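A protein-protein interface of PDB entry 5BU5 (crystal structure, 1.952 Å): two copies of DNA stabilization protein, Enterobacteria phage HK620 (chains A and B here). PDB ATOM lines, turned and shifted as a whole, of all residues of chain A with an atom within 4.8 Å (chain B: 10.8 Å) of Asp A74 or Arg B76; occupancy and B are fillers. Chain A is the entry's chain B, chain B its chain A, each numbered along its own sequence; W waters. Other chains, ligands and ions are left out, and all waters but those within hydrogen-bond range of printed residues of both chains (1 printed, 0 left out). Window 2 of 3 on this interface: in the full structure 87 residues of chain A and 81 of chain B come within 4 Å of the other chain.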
ATOM      1  N   LEU A  70      28.106 -16.828 -13.435  1.00  0.00           N
ATOM      2  CA  LEU A  70      27.381 -18.083 -13.631  1.00  0.00           C
ATOM      3  C   LEU A  70      28.046 -19.225 -12.868  1.00  0.00           C
ATOM      4  O   LEU A  70      27.368 -20.073 -12.288  1.00  0.00           O
ATOM      5  CB  LEU A  70      27.278 -18.430 -15.117  1.00  0.00           C
ATOM      6  CG  LEU A  70      26.180 -17.690 -15.878  1.00  0.00           C
ATOM      7  CD1 LEU A  70      26.359 -17.843 -17.381  1.00  0.00           C
ATOM      8  CD2 LEU A  70      24.814 -18.192 -15.441  1.00  0.00           C
ATOM      9  N   ALA A  71      29.373 -19.247 -12.879  1.00  0.00           N
ATOM     10  CA  ALA A  71      30.125 -20.241 -12.124  1.00  0.00           C
ATOM     11  C   ALA A  71      29.907 -20.038 -10.629  1.00  0.00           C
ATOM     12  O   ALA A  71      29.787 -20.999  -9.867  1.00  0.00           O
ATOM     13  CB  ALA A  71      31.599 -20.165 -12.466  1.00  0.00           C
ATOM     14  N   ASP A  72      29.865 -18.774 -10.217  1.00  0.00           N
ATOM     15  CA  ASP A  72      29.589 -18.422  -8.828  1.00  0.00           C
ATOM     16  C   ASP A  72      28.209 -18.894  -8.397  1.00  0.00           C
ATOM     17  O   ASP A  72      28.057 -19.495  -7.335  1.00  0.00           O
ATOM     18  CB  ASP A  72      29.710 -16.911  -8.624  1.00  0.00           C
ATOM     19  CG  ASP A  72      29.293 -16.475  -7.231  1.00  0.00           C
ATOM     20  OD1 ASP A  72      29.977 -16.850  -6.256  1.00  0.00           O
ATOM     21  OD2 ASP A  72      28.282 -15.746  -7.112  1.00  0.00           O
ATOM     22  N   HIS A  73      27.206 -18.616  -9.223  1.00  0.00           N
ATOM     23  CA  HIS A  73      25.842 -19.033  -8.923  1.00  0.00           C
ATOM     24  C   HIS A  73      25.737 -20.549  -8.838  1.00  0.00           C
ATOM     25  O   HIS A  73      25.056 -21.080  -7.963  1.00  0.00           O
ATOM     26  CB  HIS A  73      24.865 -18.493  -9.969  1.00  0.00           C
ATOM     27  CG  HIS A  73      24.642 -17.015  -9.879  1.00  0.00           C
ATOM     28  ND1 HIS A  73      23.794 -16.335 -10.724  1.00  0.00           N
ATOM     29  CD2 HIS A  73      25.179 -16.083  -9.056  1.00  0.00           C
ATOM     30  CE1 HIS A  73      23.806 -15.050 -10.419  1.00  0.00           C
ATOM     31  NE2 HIS A  73      24.640 -14.869  -9.410  1.00  0.00           N
ATOM     32  N   ASP A  74      26.400 -21.239  -9.763  1.00  0.00           N
ATOM     33  CA  ASP A  74      26.403 -22.699  -9.786  1.00  0.00           C
ATOM     34  C   ASP A  74      26.928 -23.291  -8.479  1.00  0.00           C
ATOM     35  O   ASP A  74      26.339 -24.219  -7.922  1.00  0.00           O
ATOM     36  CB  ASP A  74      27.241 -23.210 -10.957  1.00  0.00           C
ATOM     37  CG  ASP A  74      27.238 -24.720 -11.059  1.00  0.00           C
ATOM     38  OD1 ASP A  74      26.161 -25.298 -11.320  1.00  0.00           O
ATOM     39  OD2 ASP A  74      28.311 -25.332 -10.872  1.00  0.00           O
ATOM     40  N   ALA A  75      28.037 -22.743  -7.996  1.00  0.00           N
ATOM     41  CA  ALA A  75      28.641 -23.197  -6.751  1.00  0.00           C
ATOM     42  C   ALA A  75      27.730 -22.894  -5.567  1.00  0.00           C
ATOM     43  O   ALA A  75      27.614 -23.695  -4.639  1.00  0.00           O
ATOM     44  CB  ALA A  75      29.999 -22.553  -6.556  1.00  0.00           C
ATOM     45  N   ARG A  76      27.083 -21.735  -5.605  1.00  0.00           N
ATOM     46  CA  ARG A  76      26.201 -21.323  -4.522  1.00  0.00           C
ATOM     47  C   ARG A  76      24.922 -22.158  -4.493  1.00  0.00           C
ATOM     48  O   ARG A  76      24.452 -22.534  -3.421  1.00  0.00           O
ATOM     49  CB  ARG A  76      25.865 -19.835  -4.644  1.00  0.00           C
ATOM     50  CG  ARG A  76      27.023 -18.915  -4.278  1.00  0.00           C
ATOM     51  CD  ARG A  76      26.773 -17.492  -4.754  1.00  0.00           C
ATOM     52  NE  ARG A  76      25.585 -16.903  -4.145  1.00  0.00           N
ATOM     53  CZ  ARG A  76      24.994 -15.795  -4.584  1.00  0.00           C
ATOM     54  NH1 ARG A  76      25.471 -15.164  -5.650  1.00  0.00           N
ATOM     55  NH2 ARG A  76      23.918 -15.326  -3.967  1.00  0.00           N
ATOM     56  N   ILE A  77      24.366 -22.455  -5.664  1.00  0.00           N
ATOM     57  CA  ILE A  77      23.165 -23.283  -5.735  1.00  0.00           C
ATOM     58  C   ILE A  77      23.456 -24.685  -5.198  1.00  0.00           C
ATOM     59  O   ILE A  77      22.671 -25.239  -4.427  1.00  0.00           O
ATOM     60  CB  ILE A  77      22.622 -23.380  -7.175  1.00  0.00           C
ATOM     61  CG1 ILE A  77      22.108 -22.019  -7.646  1.00  0.00           C
ATOM     62  CG2 ILE A  77      21.495 -24.390  -7.261  1.00  0.00           C
ATOM     63  CD1 ILE A  77      21.944 -21.921  -9.148  1.00  0.00           C
ATOM     64  N   ALA A  78      24.596 -25.243  -5.595  1.00  0.00           N
ATOM     65  CA  ALA A  78      25.016 -26.559  -5.123  1.00  0.00           C
ATOM     66  C   ALA A  78      25.255 -26.569  -3.615  1.00  0.00           C
ATOM     67  O   ALA A  78      24.917 -27.540  -2.936  1.00  0.00           O
ATOM     68  CB  ALA A  78      26.272 -27.008  -5.858  1.00  0.00           C
ATOM     69  N   GLU B  65      24.657 -20.838 -24.883  1.00  0.00           N
ATOM     70  CA  GLU B  65      25.191 -21.753 -23.886  1.00  0.00           C
ATOM     71  C   GLU B  65      25.020 -21.089 -22.517  1.00  0.00           C
ATOM     72  O   GLU B  65      24.905 -21.775 -21.489  1.00  0.00           O
ATOM     73  CB  GLU B  65      26.667 -22.072 -24.167  1.00  0.00           C
ATOM     74  CG  GLU B  65      27.528 -22.270 -22.940  1.00  0.00           C
ATOM     75  CD  GLU B  65      27.250 -23.603 -22.279  1.00  0.00           C
ATOM     76  OE1 GLU B  65      26.673 -24.473 -22.959  1.00  0.00           O
ATOM     77  OE2 GLU B  65      27.589 -23.790 -21.090  1.00  0.00           O
ATOM     78  N   GLN B  66      25.010 -19.754 -22.507  1.00  0.00           N
ATOM     79  CA  GLN B  66      24.737 -19.019 -21.286  1.00  0.00           C
ATOM     80  C   GLN B  66      23.241 -19.044 -20.990  1.00  0.00           C
ATOM     81  O   GLN B  66      22.844 -19.089 -19.827  1.00  0.00           O
ATOM     82  CB  GLN B  66      25.232 -17.577 -21.384  1.00  0.00           C
ATOM     83  CG  GLN B  66      26.751 -17.405 -21.269  1.00  0.00           C
ATOM     84  CD  GLN B  66      27.195 -15.954 -21.385  1.00  0.00           C
ATOM     85  OE1 GLN B  66      26.480 -15.103 -21.914  1.00  0.00           O
ATOM     86  NE2 GLN B  66      28.376 -15.666 -20.860  1.00  0.00           N
ATOM     87  N   VAL B  68      21.211 -21.518 -21.794  1.00  0.00           N
ATOM     88  CA  VAL B  68      20.928 -22.873 -21.332  1.00  0.00           C
ATOM     89  C   VAL B  68      21.225 -23.029 -19.839  1.00  0.00           C
ATOM     90  O   VAL B  68      20.436 -23.621 -19.100  1.00  0.00           O
ATOM     91  CB  VAL B  68      21.744 -23.915 -22.128  1.00  0.00           C
ATOM     92  CG1 VAL B  68      21.710 -25.270 -21.437  1.00  0.00           C
ATOM     93  CG2 VAL B  68      21.213 -24.027 -23.549  1.00  0.00           C
ATOM     94  N   GLU B  69      22.356 -22.489 -19.395  1.00  0.00           N
ATOM     95  CA  GLU B  69      22.736 -22.590 -17.989  1.00  0.00           C
ATOM     96  C   GLU B  69      21.846 -21.724 -17.096  1.00  0.00           C
ATOM     97  O   GLU B  69      21.536 -22.107 -15.969  1.00  0.00           O
ATOM     98  CB  GLU B  69      24.205 -22.211 -17.790  1.00  0.00           C
ATOM     99  CG  GLU B  69      24.726 -22.553 -16.401  1.00  0.00           C
ATOM    100  CD  GLU B  69      26.152 -22.092 -16.167  1.00  0.00           C
ATOM    101  OE1 GLU B  69      26.700 -21.388 -17.040  1.00  0.00           O
ATOM    102  OE2 GLU B  69      26.718 -22.427 -15.102  1.00  0.00           O
ATOM    103  N   LEU B  70      21.430 -20.563 -17.595  1.00  0.00           N
ATOM    104  CA  LEU B  70      20.537 -19.702 -16.819  1.00  0.00           C
ATOM    105  C   LEU B  70      19.211 -20.408 -16.545  1.00  0.00           C
ATOM    106  O   LEU B  70      18.684 -20.343 -15.433  1.00  0.00           O
ATOM    107  CB  LEU B  70      20.295 -18.374 -17.545  1.00  0.00           C
ATOM    108  CG  LEU B  70      21.413 -17.336 -17.405  1.00  0.00           C
ATOM    109  CD1 LEU B  70      21.247 -16.213 -18.412  1.00  0.00           C
ATOM    110  CD2 LEU B  70      21.445 -16.778 -15.991  1.00  0.00           C
ATOM    111  N   ALA B  71      18.698 -21.107 -17.556  1.00  0.00           N
ATOM    112  CA  ALA B  71      17.477 -21.892 -17.414  1.00  0.00           C
ATOM    113  C   ALA B  71      17.673 -23.055 -16.439  1.00  0.00           C
ATOM    114  O   ALA B  71      16.774 -23.379 -15.658  1.00  0.00           O
ATOM    115  CB  ALA B  71      17.020 -22.406 -18.771  1.00  0.00           C
ATOM    116  N   ASP B  72      18.843 -23.689 -16.506  1.00  0.00           N
ATOM    117  CA  ASP B  72      19.198 -24.764 -15.583  1.00  0.00           C
ATOM    118  C   ASP B  72      19.254 -24.267 -14.142  1.00  0.00           C
ATOM    119  O   ASP B  72      18.714 -24.902 -13.238  1.00  0.00           O
ATOM    120  CB  ASP B  72      20.541 -25.387 -15.964  1.00  0.00           C
ATOM    121  CG  ASP B  72      21.006 -26.430 -14.959  1.00  0.00           C
ATOM    122  OD1 ASP B  72      20.344 -27.486 -14.845  1.00  0.00           O
ATOM    123  OD2 ASP B  72      22.031 -26.197 -14.283  1.00  0.00           O
ATOM    124  N   HIS B  73      19.926 -23.137 -13.936  1.00  0.00           N
ATOM    125  CA  HIS B  73      20.029 -22.540 -12.608  1.00  0.00           C
ATOM    126  C   HIS B  73      18.650 -22.173 -12.081  1.00  0.00           C
ATOM    127  O   HIS B  73      18.338 -22.416 -10.919  1.00  0.00           O
ATOM    128  CB  HIS B  73      20.932 -21.306 -12.632  1.00  0.00           C
ATOM    129  CG  HIS B  73      22.387 -21.623 -12.790  1.00  0.00           C
ATOM    130  ND1 HIS B  73      23.358 -20.648 -12.864  1.00  0.00           N
ATOM    131  CD2 HIS B  73      23.036 -22.808 -12.879  1.00  0.00           C
ATOM    132  CE1 HIS B  73      24.541 -21.217 -12.996  1.00  0.00           C
ATOM    133  NE2 HIS B  73      24.377 -22.528 -13.008  1.00  0.00           N
ATOM    134  N   ASP B  74      17.830 -21.597 -12.954  1.00  0.00           N
ATOM    135  CA  ASP B  74      16.469 -21.211 -12.606  1.00  0.00           C
ATOM    136  C   ASP B  74      15.657 -22.400 -12.096  1.00  0.00           C
ATOM    137  O   ASP B  74      14.937 -22.292 -11.103  1.00  0.00           O
ATOM    138  CB  ASP B  74      15.776 -20.575 -13.809  1.00  0.00           C
ATOM    139  CG  ASP B  74      14.376 -20.106 -13.487  1.00  0.00           C
ATOM    140  OD1 ASP B  74      14.233 -19.189 -12.651  1.00  0.00           O
ATOM    141  OD2 ASP B  74      13.417 -20.656 -14.069  1.00  0.00           O
ATOM    142  N   ALA B  75      15.766 -23.530 -12.787  1.00  0.00           N
ATOM    143  CA  ALA B  75      15.065 -24.743 -12.386  1.00  0.00           C
ATOM    144  C   ALA B  75      15.599 -25.274 -11.058  1.00  0.00           C
ATOM    145  O   ALA B  75      14.840 -25.761 -10.222  1.00  0.00           O
ATOM    146  CB  ALA B  75      15.184 -25.803 -13.464  1.00  0.00           C
ATOM    147  N   ARG B  76      16.915 -25.191 -10.877  1.00  0.00           N
ATOM    148  CA  ARG B  76      17.557 -25.662  -9.652  1.00  0.00           C
ATOM    149  C   ARG B  76      17.247 -24.743  -8.468  1.00  0.00           C
ATOM    150  O   ARG B  76      17.023 -25.212  -7.351  1.00  0.00           O
ATOM    151  CB  ARG B  76      19.067 -25.784  -9.862  1.00  0.00           C
ATOM    152  CG  ARG B  76      19.474 -26.986 -10.708  1.00  0.00           C
ATOM    153  CD  ARG B  76      20.906 -26.862 -11.218  1.00  0.00           C
ATOM    154  NE  ARG B  76      21.882 -26.765 -10.137  1.00  0.00           N
ATOM    155  CZ  ARG B  76      23.144 -26.388 -10.310  1.00  0.00           C
ATOM    156  NH1 ARG B  76      23.582 -26.079 -11.521  1.00  0.00           N
ATOM    157  NH2 ARG B  76      23.972 -26.319  -9.275  1.00  0.00           N
ATOM    158  N   ILE B  77      17.241 -23.435  -8.707  1.00  0.00           N
ATOM    159  CA  ILE B  77      16.902 -22.481  -7.654  1.00  0.00           C
ATOM    160  C   ILE B  77      15.460 -22.691  -7.211  1.00  0.00           C
ATOM    161  O   ILE B  77      15.163 -22.709  -6.013  1.00  0.00           O
ATOM    162  CB  ILE B  77      17.094 -21.026  -8.115  1.00  0.00           C
ATOM    163  CG1 ILE B  77      18.576 -20.732  -8.348  1.00  0.00           C
ATOM    164  CG2 ILE B  77      16.546 -20.061  -7.081  1.00  0.00           C
ATOM    165  CD1 ILE B  77      18.825 -19.487  -9.175  1.00  0.00           C
ATOM    166  N   ALA B  78      14.572 -22.878  -8.184  1.00  0.00           N
ATOM    167  CA  ALA B  78      13.163 -23.129  -7.908  1.00  0.00           C
ATOM    168  C   ALA B  78      12.985 -24.423  -7.120  1.00  0.00           C
ATOM    169  O   ALA B  78      12.152 -24.503  -6.214  1.00  0.00           O
ATOM    170  CB  ALA B  78      12.373 -23.185  -9.202  1.00  0.00           C
ATOM    171  N   ALA B  79      13.773 -25.434  -7.473  1.00  0.00           N
ATOM    172  CA  ALA B  79      13.755 -26.710  -6.768  1.00  0.00           C
ATOM    173  C   ALA B  79      14.213 -26.544  -5.319  1.00  0.00           C
ATOM    174  O   ALA B  79      13.639 -27.142  -4.406  1.00  0.00           O
ATOM    175  CB  ALA B  79      14.623 -27.726  -7.488  1.00  0.00           C
ATOM    176  N   ASN B  80      15.255 -25.742  -5.110  1.00  0.00           N
ATOM    177  CA  ASN B  80      15.724 -25.461  -3.756  1.00  0.00           C
ATOM    178  C   ASN B  80      14.683 -24.709  -2.938  1.00  0.00           C
ATOM    179  O   ASN B  80      14.476 -24.998  -1.762  1.00  0.00           O
ATOM    180  CB  ASN B  80      17.030 -24.666  -3.784  1.00  0.00           C
ATOM    181  CG  ASN B  80      18.229 -25.535  -4.100  1.00  0.00           C
ATOM    182  OD1 ASN B  80      18.121 -26.757  -4.162  1.00  0.00           O
ATOM    183  ND2 ASN B  80      19.388 -24.909  -4.270  1.00  0.00           N
ATOM    184  N   THR B  81      14.033 -23.739  -3.569  1.00  0.00           N
ATOM    185  CA  THR B  81      12.992 -22.950  -2.915  1.00  0.00           C
ATOM    186  C   THR B  81      11.833 -23.845  -2.483  1.00  0.00           C
ATOM    187  O   THR B  81      11.288 -23.698  -1.386  1.00  0.00           O
ATOM    188  CB  THR B  81      12.463 -21.841  -3.837  1.00  0.00           C
ATOM    189  OG1 THR B  81      13.537 -20.965  -4.199  1.00  0.00           O
ATOM    190  CG2 THR B  81      11.365 -21.041  -3.144  1.00  0.00           C
ATOM    191  N   LYS B  82      11.474 -24.785  -3.352  1.00  0.00           N
ATOM    192  CA  LYS B  82      10.377 -25.700  -3.086  1.00  0.00           C
ATOM    193  C   LYS B  82      10.743 -26.648  -1.958  1.00  0.00           C
ATOM    194  O   LYS B  82       9.920 -26.954  -1.095  1.00  0.00           O
ATOM    195  CB  LYS B  82      10.043 -26.502  -4.346  1.00  0.00           C
ATOM    196  CG  LYS B  82       8.765 -27.324  -4.275  1.00  0.00           C
ATOM    197  CD  LYS B  82       8.549 -28.101  -5.569  1.00  0.00           C
ATOM    198  CE  LYS B  82       7.447 -27.497  -6.427  1.00  0.00           C
ATOM    199  NZ  LYS B  82       6.142 -27.435  -5.710  1.00  0.00           N
ATOM    200  N   ALA B  83      12.000 -27.074  -1.951  1.00  0.00           N
ATOM    201  CA  ALA B  83      12.503 -27.959  -0.914  1.00  0.00           C
ATOM    202  C   ALA B  83      12.548 -27.247   0.431  1.00  0.00           C
ATOM    203  O   ALA B  83      12.211 -27.828   1.461  1.00  0.00           O
ATOM    204  CB  ALA B  83      13.881 -28.483  -1.290  1.00  0.00           C
ATOM    205  N   ILE B  84      12.955 -25.982   0.418  1.00  0.00           N
ATOM    206  CA  ILE B  84      12.997 -25.184   1.640  1.00  0.00           C
ATOM    207  C   ILE B  84      11.601 -25.029   2.235  1.00  0.00           C
ATOM    208  O   ILE B  84      11.406 -25.191   3.440  1.00  0.00           O
ATOM    209  CB  ILE B  84      13.610 -23.792   1.385  1.00  0.00           C
ATOM    210  CG1 ILE B  84      15.116 -23.908   1.152  1.00  0.00           C
ATOM    211  CG2 ILE B  84      13.347 -22.864   2.558  1.00  0.00           C
ATOM    212  CD1 ILE B  84      15.735 -22.660   0.551  1.00  0.00           C
HETATM  213  O   HOH W   1      22.344 -18.051 -12.243  1.00  0.00           O
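Ala A71 touches none of the printed residues of chain B. His A73 touches one residue of chain B. Of chain B, only His B73 (3.6 Å) and Arg B76 (2.7 Å) come within 4 Å of Asp A74. No residue of chain B comes within 4 Å of Ala A75. Ile A77 touches four residues of chain B. Of chain B, only Arg B76 comes within 4 Å of Ala A78. Of the printed residues of chain A, Leu B70 touches Leu A70 (3.7 Å). Asp B74 touches none of the printed residues of chain A. Arg B76 touches just these residues of chain A: Asp A74 (2.7 Å), Ile A77 (3.7 Å) and Ala A78 (3.9 Å). Of the printed residues of chain A, Ile B77 touches Ile A77. Of the printed residues of chain A, Asn B80 touches Ile A77. Lys B82 touches none of the printed residues of chain A. The nearest printed residue of chain A that does not touch Arg B76 is His A73 (5.5 Å). The nearest printed residue of chain A that does not touch His B73 is Ala A71 (5.2 Å).
Hydrophobic or aromatic side chains of chain B that line the printed part of chain A: Leu B70, His B73 and Ile B77. Along chain B the printed residues that touch a printed residue of chain A span positions 66 to 80. Printed residues of chain A that touch a printed residue of chain B: Leu A70, His A73, Asp A74, Ile A77 and Ala A78. Among the printed residues, 12 pairs touch across the chains.
Among the printed residues, merely in contact across the chains: Leu A70 with Gln B66 (3.9 Å), Leu A70 with Glu B69 (3.6 Å), Leu A70 with Leu B70 (3.7 Å), Leu A70 with His B73 (3.1 Å), His A73 with His B73 (3.9 Å), Asp A74 with His B73 (3.6 Å), Ile A77 with His B73 (3.7 Å), Ile A77 with Arg B76 (3.7 Å), Ile A77 with Ile B77 (3.7 Å) and Ala A78 with Arg B76 (3.9 Å).
Water W1 bridges ND1 of His A73 and ND1 of His B73.
NE2 of His B73 lies within hydrogen-bond range of OE2 of Glu B69, 3.1 Å away. The backbone carbonyl oxygen (O) of Ile B77 sits at hydrogen-bond distance from the side-chain hydroxyl (OG1) of Thr B81 (3.0 Å). The guanidinium group of Arg B76 lies within salt-bridge range of the side-chain carboxylate of Asp B72, 3.2 Å away.
Leu A70 touches its own counterpart, Leu B70. His B73 touches its own counterpart, His A73. Ile A77 touches His B73, but with the chains exchanged His A73 does not touch Ile B77 (6.1 Å). Ile A77 touches its own counterpart, Ile B77. 9 positions are printed for both chains.
OD1 of Asp A74 lies within salt-bridge range of NH1 of Arg B76. The side-chain amide nitrogen of Asn B80 is in hydrogen-bond range of the backbone carbonyl oxygen of Ile A77 (3.3 Å).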
